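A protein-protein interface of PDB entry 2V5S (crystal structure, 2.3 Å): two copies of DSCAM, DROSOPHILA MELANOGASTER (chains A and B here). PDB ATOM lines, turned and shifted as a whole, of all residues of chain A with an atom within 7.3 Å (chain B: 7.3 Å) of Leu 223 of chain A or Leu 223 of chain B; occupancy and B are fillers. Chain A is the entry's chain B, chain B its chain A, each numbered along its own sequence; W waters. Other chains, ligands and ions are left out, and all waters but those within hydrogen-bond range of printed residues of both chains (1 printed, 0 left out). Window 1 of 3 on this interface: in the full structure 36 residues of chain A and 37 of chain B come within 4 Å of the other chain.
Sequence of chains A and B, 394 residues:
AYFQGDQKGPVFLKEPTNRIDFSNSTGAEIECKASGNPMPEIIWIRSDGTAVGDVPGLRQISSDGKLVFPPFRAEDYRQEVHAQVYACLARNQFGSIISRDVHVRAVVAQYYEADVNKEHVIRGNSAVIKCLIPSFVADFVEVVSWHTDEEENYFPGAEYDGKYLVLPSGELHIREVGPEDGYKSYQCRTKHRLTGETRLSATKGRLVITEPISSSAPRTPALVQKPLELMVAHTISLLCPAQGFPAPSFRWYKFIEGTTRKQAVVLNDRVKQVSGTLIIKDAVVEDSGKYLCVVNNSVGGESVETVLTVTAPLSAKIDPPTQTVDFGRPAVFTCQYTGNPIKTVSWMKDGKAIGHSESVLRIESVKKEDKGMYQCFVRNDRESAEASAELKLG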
ATOM      1  N   LYS A 130      -5.250 -11.102   5.196  1.00  0.00           N
ATOM      2  CA  LYS A 130      -4.980  -9.683   5.340  1.00  0.00           C
ATOM      3  C   LYS A 130      -5.465  -8.944   4.103  1.00  0.00           C
ATOM      4  O   LYS A 130      -5.358  -9.433   2.993  1.00  0.00           O
ATOM      5  CB  LYS A 130      -3.469  -9.440   5.341  1.00  0.00           C
ATOM      6  CG  LYS A 130      -2.964  -8.484   6.424  1.00  0.00           C
ATOM      7  CD  LYS A 130      -3.810  -7.207   6.683  1.00  0.00           C
ATOM      8  CE  LYS A 130      -3.103  -6.269   7.681  1.00  0.00           C
ATOM      9  NZ  LYS A 130      -3.866  -5.315   8.549  1.00  0.00           N
ATOM     10  N   GLU A 171      -8.535  -7.801   9.781  1.00  0.00           N
ATOM     11  CA  GLU A 171      -8.169  -9.080   9.158  1.00  0.00           C
ATOM     12  C   GLU A 171      -9.322 -10.084   9.267  1.00  0.00           C
ATOM     13  O   GLU A 171     -10.190  -9.954  10.120  1.00  0.00           O
ATOM     14  CB  GLU A 171      -6.943  -9.650   9.851  1.00  0.00           C
ATOM     15  CG  GLU A 171      -5.739  -8.720   9.891  1.00  0.00           C
ATOM     16  CD  GLU A 171      -5.644  -7.921  11.180  1.00  0.00           C
ATOM     17  OE1 GLU A 171      -6.647  -7.772  11.937  1.00  0.00           O
ATOM     18  OE2 GLU A 171      -4.527  -7.372  11.326  1.00  0.00           O
ATOM     19  N   THR A 220       6.837 -18.224  14.250  1.00  0.00           N
ATOM     20  CA  THR A 220       6.350 -16.847  14.130  1.00  0.00           C
ATOM     21  C   THR A 220       7.176 -16.152  13.042  1.00  0.00           C
ATOM     22  O   THR A 220       8.351 -16.468  12.884  1.00  0.00           O
ATOM     23  CB  THR A 220       6.609 -16.025  15.441  1.00  0.00           C
ATOM     24  OG1 THR A 220       8.008 -16.086  15.806  1.00  0.00           O
ATOM     25  CG2 THR A 220       5.783 -16.590  16.576  1.00  0.00           C
ATOM     26  N   PRO A 221       6.621 -15.121  12.380  1.00  0.00           N
ATOM     27  CA  PRO A 221       7.299 -14.450  11.262  1.00  0.00           C
ATOM     28  C   PRO A 221       8.364 -13.418  11.627  1.00  0.00           C
ATOM     29  O   PRO A 221       8.416 -12.890  12.738  1.00  0.00           O
ATOM     30  CB  PRO A 221       6.159 -13.752  10.505  1.00  0.00           C
ATOM     31  CG  PRO A 221       4.954 -13.833  11.369  1.00  0.00           C
ATOM     32  CD  PRO A 221       5.329 -14.487  12.680  1.00  0.00           C
ATOM     33  N   ALA A 222       9.185 -13.073  10.648  1.00  0.00           N
ATOM     34  CA  ALA A 222      10.217 -12.089  10.921  1.00  0.00           C
ATOM     35  C   ALA A 222       9.597 -10.724  11.241  1.00  0.00           C
ATOM     36  O   ALA A 222      10.078 -10.025  12.126  1.00  0.00           O
ATOM     37  CB  ALA A 222      11.242 -11.983   9.765  1.00  0.00           C
ATOM     38  N   LEU A 223       8.604 -10.281  10.478  1.00  0.00           N
ATOM     39  CA  LEU A 223       8.152  -8.899  10.629  1.00  0.00           C
ATOM     40  C   LEU A 223       7.084  -8.951  11.697  1.00  0.00           C
ATOM     41  O   LEU A 223       6.175  -9.750  11.562  1.00  0.00           O
ATOM     42  CB  LEU A 223       7.623  -8.273   9.327  1.00  0.00           C
ATOM     43  CG  LEU A 223       8.547  -8.332   8.127  1.00  0.00           C
ATOM     44  CD1 LEU A 223       7.853  -7.917   6.831  1.00  0.00           C
ATOM     45  CD2 LEU A 223       9.798  -7.503   8.404  1.00  0.00           C
ATOM     46  N   VAL A 224       7.162  -8.143  12.746  1.00  0.00           N
ATOM     47  CA  VAL A 224       6.096  -8.125  13.750  1.00  0.00           C
ATOM     48  C   VAL A 224       5.532  -6.742  14.040  1.00  0.00           C
ATOM     49  O   VAL A 224       6.147  -5.731  13.743  1.00  0.00           O
ATOM     50  CB  VAL A 224       6.588  -8.629  15.093  1.00  0.00           C
ATOM     51  CG1 VAL A 224       7.252 -10.001  14.946  1.00  0.00           C
ATOM     52  CG2 VAL A 224       7.517  -7.591  15.656  1.00  0.00           C
ATOM     53  N   GLN A 225       4.341  -6.692  14.620  1.00  0.00           N
ATOM     54  CA  GLN A 225       3.623  -5.437  14.840  1.00  0.00           C
ATOM     55  C   GLN A 225       4.404  -4.456  15.709  1.00  0.00           C
ATOM     56  O   GLN A 225       4.691  -4.725  16.876  1.00  0.00           O
ATOM     57  CB  GLN A 225       2.276  -5.739  15.491  1.00  0.00           C
ATOM     58  CG  GLN A 225       1.333  -4.546  15.865  1.00  0.00           C
ATOM     59  CD  GLN A 225       1.134  -3.573  14.699  1.00  0.00           C
ATOM     60  OE1 GLN A 225       0.443  -3.901  13.735  1.00  0.00           O
ATOM     61  NE2 GLN A 225       1.804  -2.419  14.728  1.00  0.00           N
ATOM     62  N   LYS A 226       4.742  -3.295  15.161  1.00  0.00           N
ATOM     63  CA  LYS A 226       5.339  -2.223  15.959  1.00  0.00           C
ATOM     64  C   LYS A 226       4.379  -1.590  16.973  1.00  0.00           C
ATOM     65  O   LYS A 226       3.170  -1.820  16.931  1.00  0.00           O
ATOM     66  CB  LYS A 226       5.852  -1.110  15.043  1.00  0.00           C
ATOM     67  CG  LYS A 226       4.778  -0.153  14.535  1.00  0.00           C
ATOM     68  CD  LYS A 226       5.123   0.414  13.183  1.00  0.00           C
ATOM     69  CE  LYS A 226       4.437   1.753  12.967  1.00  0.00           C
ATOM     70  NZ  LYS A 226       5.067   2.510  11.822  1.00  0.00           N
ATOM     71  N   LEU A 239      -2.524  -9.774  17.633  1.00  0.00           N
ATOM     72  CA  LEU A 239      -2.402 -11.003  16.886  1.00  0.00           C
ATOM     73  C   LEU A 239      -1.128 -11.700  17.313  1.00  0.00           C
ATOM     74  O   LEU A 239      -0.166 -11.031  17.690  1.00  0.00           O
ATOM     75  CB  LEU A 239      -2.368 -10.669  15.395  1.00  0.00           C
ATOM     76  CG  LEU A 239      -3.716 -10.347  14.736  1.00  0.00           C
ATOM     77  CD1 LEU A 239      -4.209  -8.918  14.984  1.00  0.00           C
ATOM     78  CD2 LEU A 239      -3.665 -10.616  13.245  1.00  0.00           C
ATOM     79  N   PRO A 241       0.815 -14.459  15.273  1.00  0.00           N
ATOM     80  CA  PRO A 241       0.856 -15.306  14.107  1.00  0.00           C
ATOM     81  C   PRO A 241       1.920 -16.392  14.309  1.00  0.00           C
ATOM     82  O   PRO A 241       3.056 -16.143  14.736  1.00  0.00           O
ATOM     83  CB  PRO A 241       1.120 -14.308  12.975  1.00  0.00           C
ATOM     84  CG  PRO A 241       1.116 -12.962  13.609  1.00  0.00           C
ATOM     85  CD  PRO A 241       1.515 -13.197  15.017  1.00  0.00           C
ATOM     86  N   VAL A 304       6.061 -13.532  20.770  1.00  0.00           N
ATOM     87  CA  VAL A 304       5.944 -12.219  20.127  1.00  0.00           C
ATOM     88  C   VAL A 304       5.544 -11.232  21.224  1.00  0.00           C
ATOM     89  O   VAL A 304       4.517 -11.442  21.869  1.00  0.00           O
ATOM     90  CB  VAL A 304       4.885 -12.278  18.978  1.00  0.00           C
ATOM     91  CG1 VAL A 304       3.948 -11.047  18.823  1.00  0.00           C
ATOM     92  CG2 VAL A 304       5.586 -12.499  17.655  1.00  0.00           C
ATOM     93  N   LYS B 130       9.786  -8.568  -2.381  1.00  0.00           N
ATOM     94  CA  LYS B 130       9.994  -9.663  -1.459  1.00  0.00           C
ATOM     95  C   LYS B 130       9.546 -10.965  -2.073  1.00  0.00           C
ATOM     96  O   LYS B 130       8.517 -11.034  -2.716  1.00  0.00           O
ATOM     97  CB  LYS B 130       9.045  -9.456  -0.303  1.00  0.00           C
ATOM     98  CG  LYS B 130       9.628  -9.671   1.080  1.00  0.00           C
ATOM     99  CD  LYS B 130       9.693 -11.150   1.433  1.00  0.00           C
ATOM    100  CE  LYS B 130      10.074 -11.317   2.887  1.00  0.00           C
ATOM    101  NZ  LYS B 130      11.513 -11.038   3.177  1.00  0.00           N
ATOM    102  N   GLU B 171      15.952  -9.914  -0.474  1.00  0.00           N
ATOM    103  CA  GLU B 171      15.053  -9.034  -1.215  1.00  0.00           C
ATOM    104  C   GLU B 171      15.721  -8.389  -2.416  1.00  0.00           C
ATOM    105  O   GLU B 171      16.958  -8.286  -2.489  1.00  0.00           O
ATOM    106  CB  GLU B 171      14.616  -7.878  -0.318  1.00  0.00           C
ATOM    107  CG  GLU B 171      13.821  -8.278   0.919  1.00  0.00           C
ATOM    108  CD  GLU B 171      14.674  -8.404   2.163  1.00  0.00           C
ATOM    109  OE1 GLU B 171      15.897  -8.262   2.016  1.00  0.00           O
ATOM    110  OE2 GLU B 171      14.154  -8.584   3.293  1.00  0.00           O
ATOM    111  N   THR B 220       5.767   4.450   7.314  1.00  0.00           N
ATOM    112  CA  THR B 220       6.415   3.150   7.459  1.00  0.00           C
ATOM    113  C   THR B 220       5.353   2.101   7.775  1.00  0.00           C
ATOM    114  O   THR B 220       4.252   2.429   8.211  1.00  0.00           O
ATOM    115  CB  THR B 220       7.491   3.194   8.569  1.00  0.00           C
ATOM    116  OG1 THR B 220       6.924   3.687   9.793  1.00  0.00           O
ATOM    117  CG2 THR B 220       8.608   4.143   8.187  1.00  0.00           C
ATOM    118  N   PRO B 221       5.667   0.822   7.513  1.00  0.00           N
ATOM    119  CA  PRO B 221       4.659  -0.218   7.736  1.00  0.00           C
ATOM    120  C   PRO B 221       4.251  -0.488   9.178  1.00  0.00           C
ATOM    121  O   PRO B 221       5.030  -0.219  10.092  1.00  0.00           O
ATOM    122  CB  PRO B 221       5.310  -1.484   7.172  1.00  0.00           C
ATOM    123  CG  PRO B 221       6.535  -1.034   6.399  1.00  0.00           C
ATOM    124  CD  PRO B 221       6.936   0.291   6.974  1.00  0.00           C
ATOM    125  N   ALA B 222       3.074  -1.090   9.342  1.00  0.00           N
ATOM    126  CA  ALA B 222       2.678  -1.723  10.601  1.00  0.00           C
ATOM    127  C   ALA B 222       3.619  -2.833  11.096  1.00  0.00           C
ATOM    128  O   ALA B 222       3.880  -2.956  12.294  1.00  0.00           O
ATOM    129  CB  ALA B 222       1.227  -2.225  10.515  1.00  0.00           C
ATOM    130  N   LEU B 223       4.155  -3.676  10.222  1.00  0.00           N
ATOM    131  CA  LEU B 223       4.926  -4.816  10.723  1.00  0.00           C
ATOM    132  C   LEU B 223       6.410  -4.534  10.512  1.00  0.00           C
ATOM    133  O   LEU B 223       6.831  -4.087   9.453  1.00  0.00           O
ATOM    134  CB  LEU B 223       4.450  -6.147  10.117  1.00  0.00           C
ATOM    135  CG  LEU B 223       2.969  -6.493  10.310  1.00  0.00           C
ATOM    136  CD1 LEU B 223       2.336  -7.277   9.161  1.00  0.00           C
ATOM    137  CD2 LEU B 223       2.693  -7.268  11.601  1.00  0.00           C
ATOM    138  N   VAL B 224       7.226  -4.737  11.536  1.00  0.00           N
ATOM    139  CA  VAL B 224       8.634  -4.410  11.443  1.00  0.00           C
ATOM    140  C   VAL B 224       9.546  -5.552  11.874  1.00  0.00           C
ATOM    141  O   VAL B 224       9.170  -6.436  12.632  1.00  0.00           O
ATOM    142  CB  VAL B 224       8.918  -3.138  12.247  1.00  0.00           C
ATOM    143  CG1 VAL B 224       8.011  -2.007  11.758  1.00  0.00           C
ATOM    144  CG2 VAL B 224       8.722  -3.332  13.726  1.00  0.00           C
ATOM    145  N   GLN B 225      10.767  -5.558  11.345  1.00  0.00           N
ATOM    146  CA  GLN B 225      11.705  -6.643  11.592  1.00  0.00           C
ATOM    147  C   GLN B 225      11.884  -6.736  13.098  1.00  0.00           C
ATOM    148  O   GLN B 225      12.179  -5.731  13.742  1.00  0.00           O
ATOM    149  CB  GLN B 225      13.024  -6.359  10.857  1.00  0.00           C
ATOM    150  CG  GLN B 225      14.147  -7.343  11.093  1.00  0.00           C
ATOM    151  CD  GLN B 225      13.657  -8.752  10.926  1.00  0.00           C
ATOM    152  OE1 GLN B 225      13.109  -9.085   9.871  1.00  0.00           O
ATOM    153  NE2 GLN B 225      13.761  -9.557  11.989  1.00  0.00           N
ATOM    154  N   LYS B 226      11.629  -7.911  13.662  1.00  0.00           N
ATOM    155  CA  LYS B 226      11.935  -8.179  15.063  1.00  0.00           C
ATOM    156  C   LYS B 226      13.423  -8.412  15.288  1.00  0.00           C
ATOM    157  O   LYS B 226      14.189  -8.515  14.331  1.00  0.00           O
ATOM    158  CB  LYS B 226      11.187  -9.413  15.561  1.00  0.00           C
ATOM    159  CG  LYS B 226      11.486 -10.709  14.832  1.00  0.00           C
ATOM    160  CD  LYS B 226      10.550 -11.802  15.289  1.00  0.00           C
ATOM    161  CE  LYS B 226      11.137 -13.193  15.215  1.00  0.00           C
ATOM    162  NZ  LYS B 226      10.393 -14.278  15.920  1.00  0.00           N
ATOM    163  N   LEU B 239      16.539  -3.076   6.798  1.00  0.00           N
ATOM    164  CA  LEU B 239      15.618  -2.413   5.901  1.00  0.00           C
ATOM    165  C   LEU B 239      14.964  -1.259   6.637  1.00  0.00           C
ATOM    166  O   LEU B 239      14.823  -1.329   7.849  1.00  0.00           O
ATOM    167  CB  LEU B 239      14.573  -3.404   5.414  1.00  0.00           C
ATOM    168  CG  LEU B 239      14.944  -4.216   4.175  1.00  0.00           C
ATOM    169  CD1 LEU B 239      15.961  -5.290   4.508  1.00  0.00           C
ATOM    170  CD2 LEU B 239      13.561  -4.724   3.796  1.00  0.00           C
ATOM    171  N   PRO B 241      11.699   0.474   5.475  1.00  0.00           N
ATOM    172  CA  PRO B 241      10.693   0.682   4.449  1.00  0.00           C
ATOM    173  C   PRO B 241       9.951   1.994   4.712  1.00  0.00           C
ATOM    174  O   PRO B 241       9.595   2.318   5.849  1.00  0.00           O
ATOM    175  CB  PRO B 241       9.818  -0.566   4.568  1.00  0.00           C
ATOM    176  CG  PRO B 241      10.525  -1.476   5.531  1.00  0.00           C
ATOM    177  CD  PRO B 241      11.336  -0.606   6.402  1.00  0.00           C
ATOM    178  N   VAL B 304      11.715   3.891  12.440  1.00  0.00           N
ATOM    179  CA  VAL B 304      11.600   2.557  13.029  1.00  0.00           C
ATOM    180  C   VAL B 304      12.917   2.062  13.635  1.00  0.00           C
ATOM    181  O   VAL B 304      14.011   2.355  13.128  1.00  0.00           O
ATOM    182  CB  VAL B 304      11.016   1.509  12.035  1.00  0.00           C
ATOM    183  CG1 VAL B 304       9.622   1.963  11.550  1.00  0.00           C
ATOM    184  CG2 VAL B 304      11.980   1.188  10.887  1.00  0.00           C
HETATM  185  O   HOH W   1       8.102 -13.373  16.659  1.00  0.00           O
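Among the printed residues, merely in contact across the chains: Leu 223 of chain A with Val 224 of chain B (3.3 Å), Val 224 of chain A with Leu 223 of chain B (3.4 Å), Ala 222 of chain A with Gln 225 of chain B (3.4 Å), Gln 225 of chain A with Leu 223 of chain B (3.5 Å), Pro 221 of chain A with Lys 226 of chain B (3.5 Å), Leu 223 of chain A with Gln 225 of chain B (3.7 Å), Ala 222 of chain A with Val 224 of chain B (3.7 Å), Val 224 of chain A with Lys 226 of chain B (3.8 Å), Lys 226 of chain A with Val 224 of chain B (3.9 Å), Val 224 of chain A with Ala 222 of chain B (3.9 Å) and Leu 223 of chain A with Leu 223 of chain B (3.9 Å).
The side-chain amino group (NZ) of Lys 226 of chain A is in hydrogen-bond range of the side-chain hydroxyl (OG1) of Thr 220 of chain B (3.0 Å).
The side-chain amino group (NZ) of Lys 226 of chain A lies close to the backbone carbonyl oxygen (O) of Pro 221 of chain B.
The side-chain hydroxyl (OG1) of Thr 220 of chain A is in hydrogen-bond range of the side-chain amino group (NZ) of Lys 226 of chain B, 3.0 Å away.
The backbone carbonyl oxygen (O) of Ala 222 of chain A sits at hydrogen-bond distance from the backbone NH (N) of Lys 226 of chain B (3.0 Å).
NE2 of Gln 225 of chain A sits at hydrogen-bond distance from O of Ala 222 of chain B, 3.2 Å away.
O of Ala 222 of chain B lies within hydrogen-bond range of N of Lys 226 of chain A (3.0 Å).
N of Val 224 of chain A is in hydrogen-bond range of O of Val 224 of chain B.
Ala 222 of chain A touches Val 224 of chain B, and with the chains exchanged Val 224 of chain A touches Ala 222 of chain B.
Ala 222 of chain A touches Gln 225 of chain B, and with the chains exchanged Gln 225 of chain A touches Ala 222 of chain B.
Leu 223 of chain A touches Gln 225 of chain B, and with the chains exchanged Gln 225 of chain A touches Leu 223 of chain B.
Val 224 of chain A touches Lys 226 of chain B, and with the chains exchanged Lys 226 of chain A touches Val 224 of chain B.
Positions printed for both chains: 130, 171, 220, 221, 222, 223, 224, 225, 226, 239, 241 and 304.
Of the 18 pairs that touch across the chains among the printed residues, 18 have their exchanged pair printed and touching as well.
Water W1 bridges the side-chain amino group of Lys 226 of chain B (2.6 Å) and the side-chain hydroxyl of Thr 220 of chain A (2.8 Å).
Leu 223 of chain A touches just these residues of chain B: Leu 223, Val 224 and Gln 225.
Of the printed residues of chain A, Leu 223 of chain B touches Leu 223 (3.9 Å), Val 224 (3.4 Å) and Gln 225 (3.5 Å).
Ala 222 of chain A touches just these residues of chain B: Val 224 (3.7 Å), Gln 225 (3.4 Å) and Lys 226 (3.0 Å).
Printed residues of chain A within 4 Å of Pro 221 of chain B: Lys 226.
Of the printed residues of chain B, Pro 221 of chain A touches Lys 226 (3.5 Å).
Of the printed residues of chain A, Lys 226 of chain B touches Thr 220 (3.0 Å), Pro 221 (3.5 Å), Ala 222 (3.0 Å) and Val 224 (3.8 Å).
Of the printed residues of chain A, Val 224 of chain B touches Ala 222, Leu 223, Val 224 and Lys 226.
Pro 241 of chain A touches none of the printed residues of chain B.
The nearest residue of chain B that does not touch Leu 223 of chain A is Lys 226 of chain B (4.7 Å).
The nearest printed residue of chain A that does not touch Ala 222 of chain B is Lys 130 of chain A (6.3 Å).
Of the 12 printed residues of chain A, 7 touch a printed residue of chain B.
Hydrophobic or aromatic side chains of chain A within 4 Å of the printed part of chain B: Ala 222, Leu 223 and Val 224.
Hydrophobic or aromatic side chains of chain B within 4 Å of the printed part of chain A: Ala 222, Leu 223 and Val 224.
Among the printed residues, no Asp or Glu carboxylate lies within 4 Å of a Lys or Arg side-chain nitrogen of the other chain.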
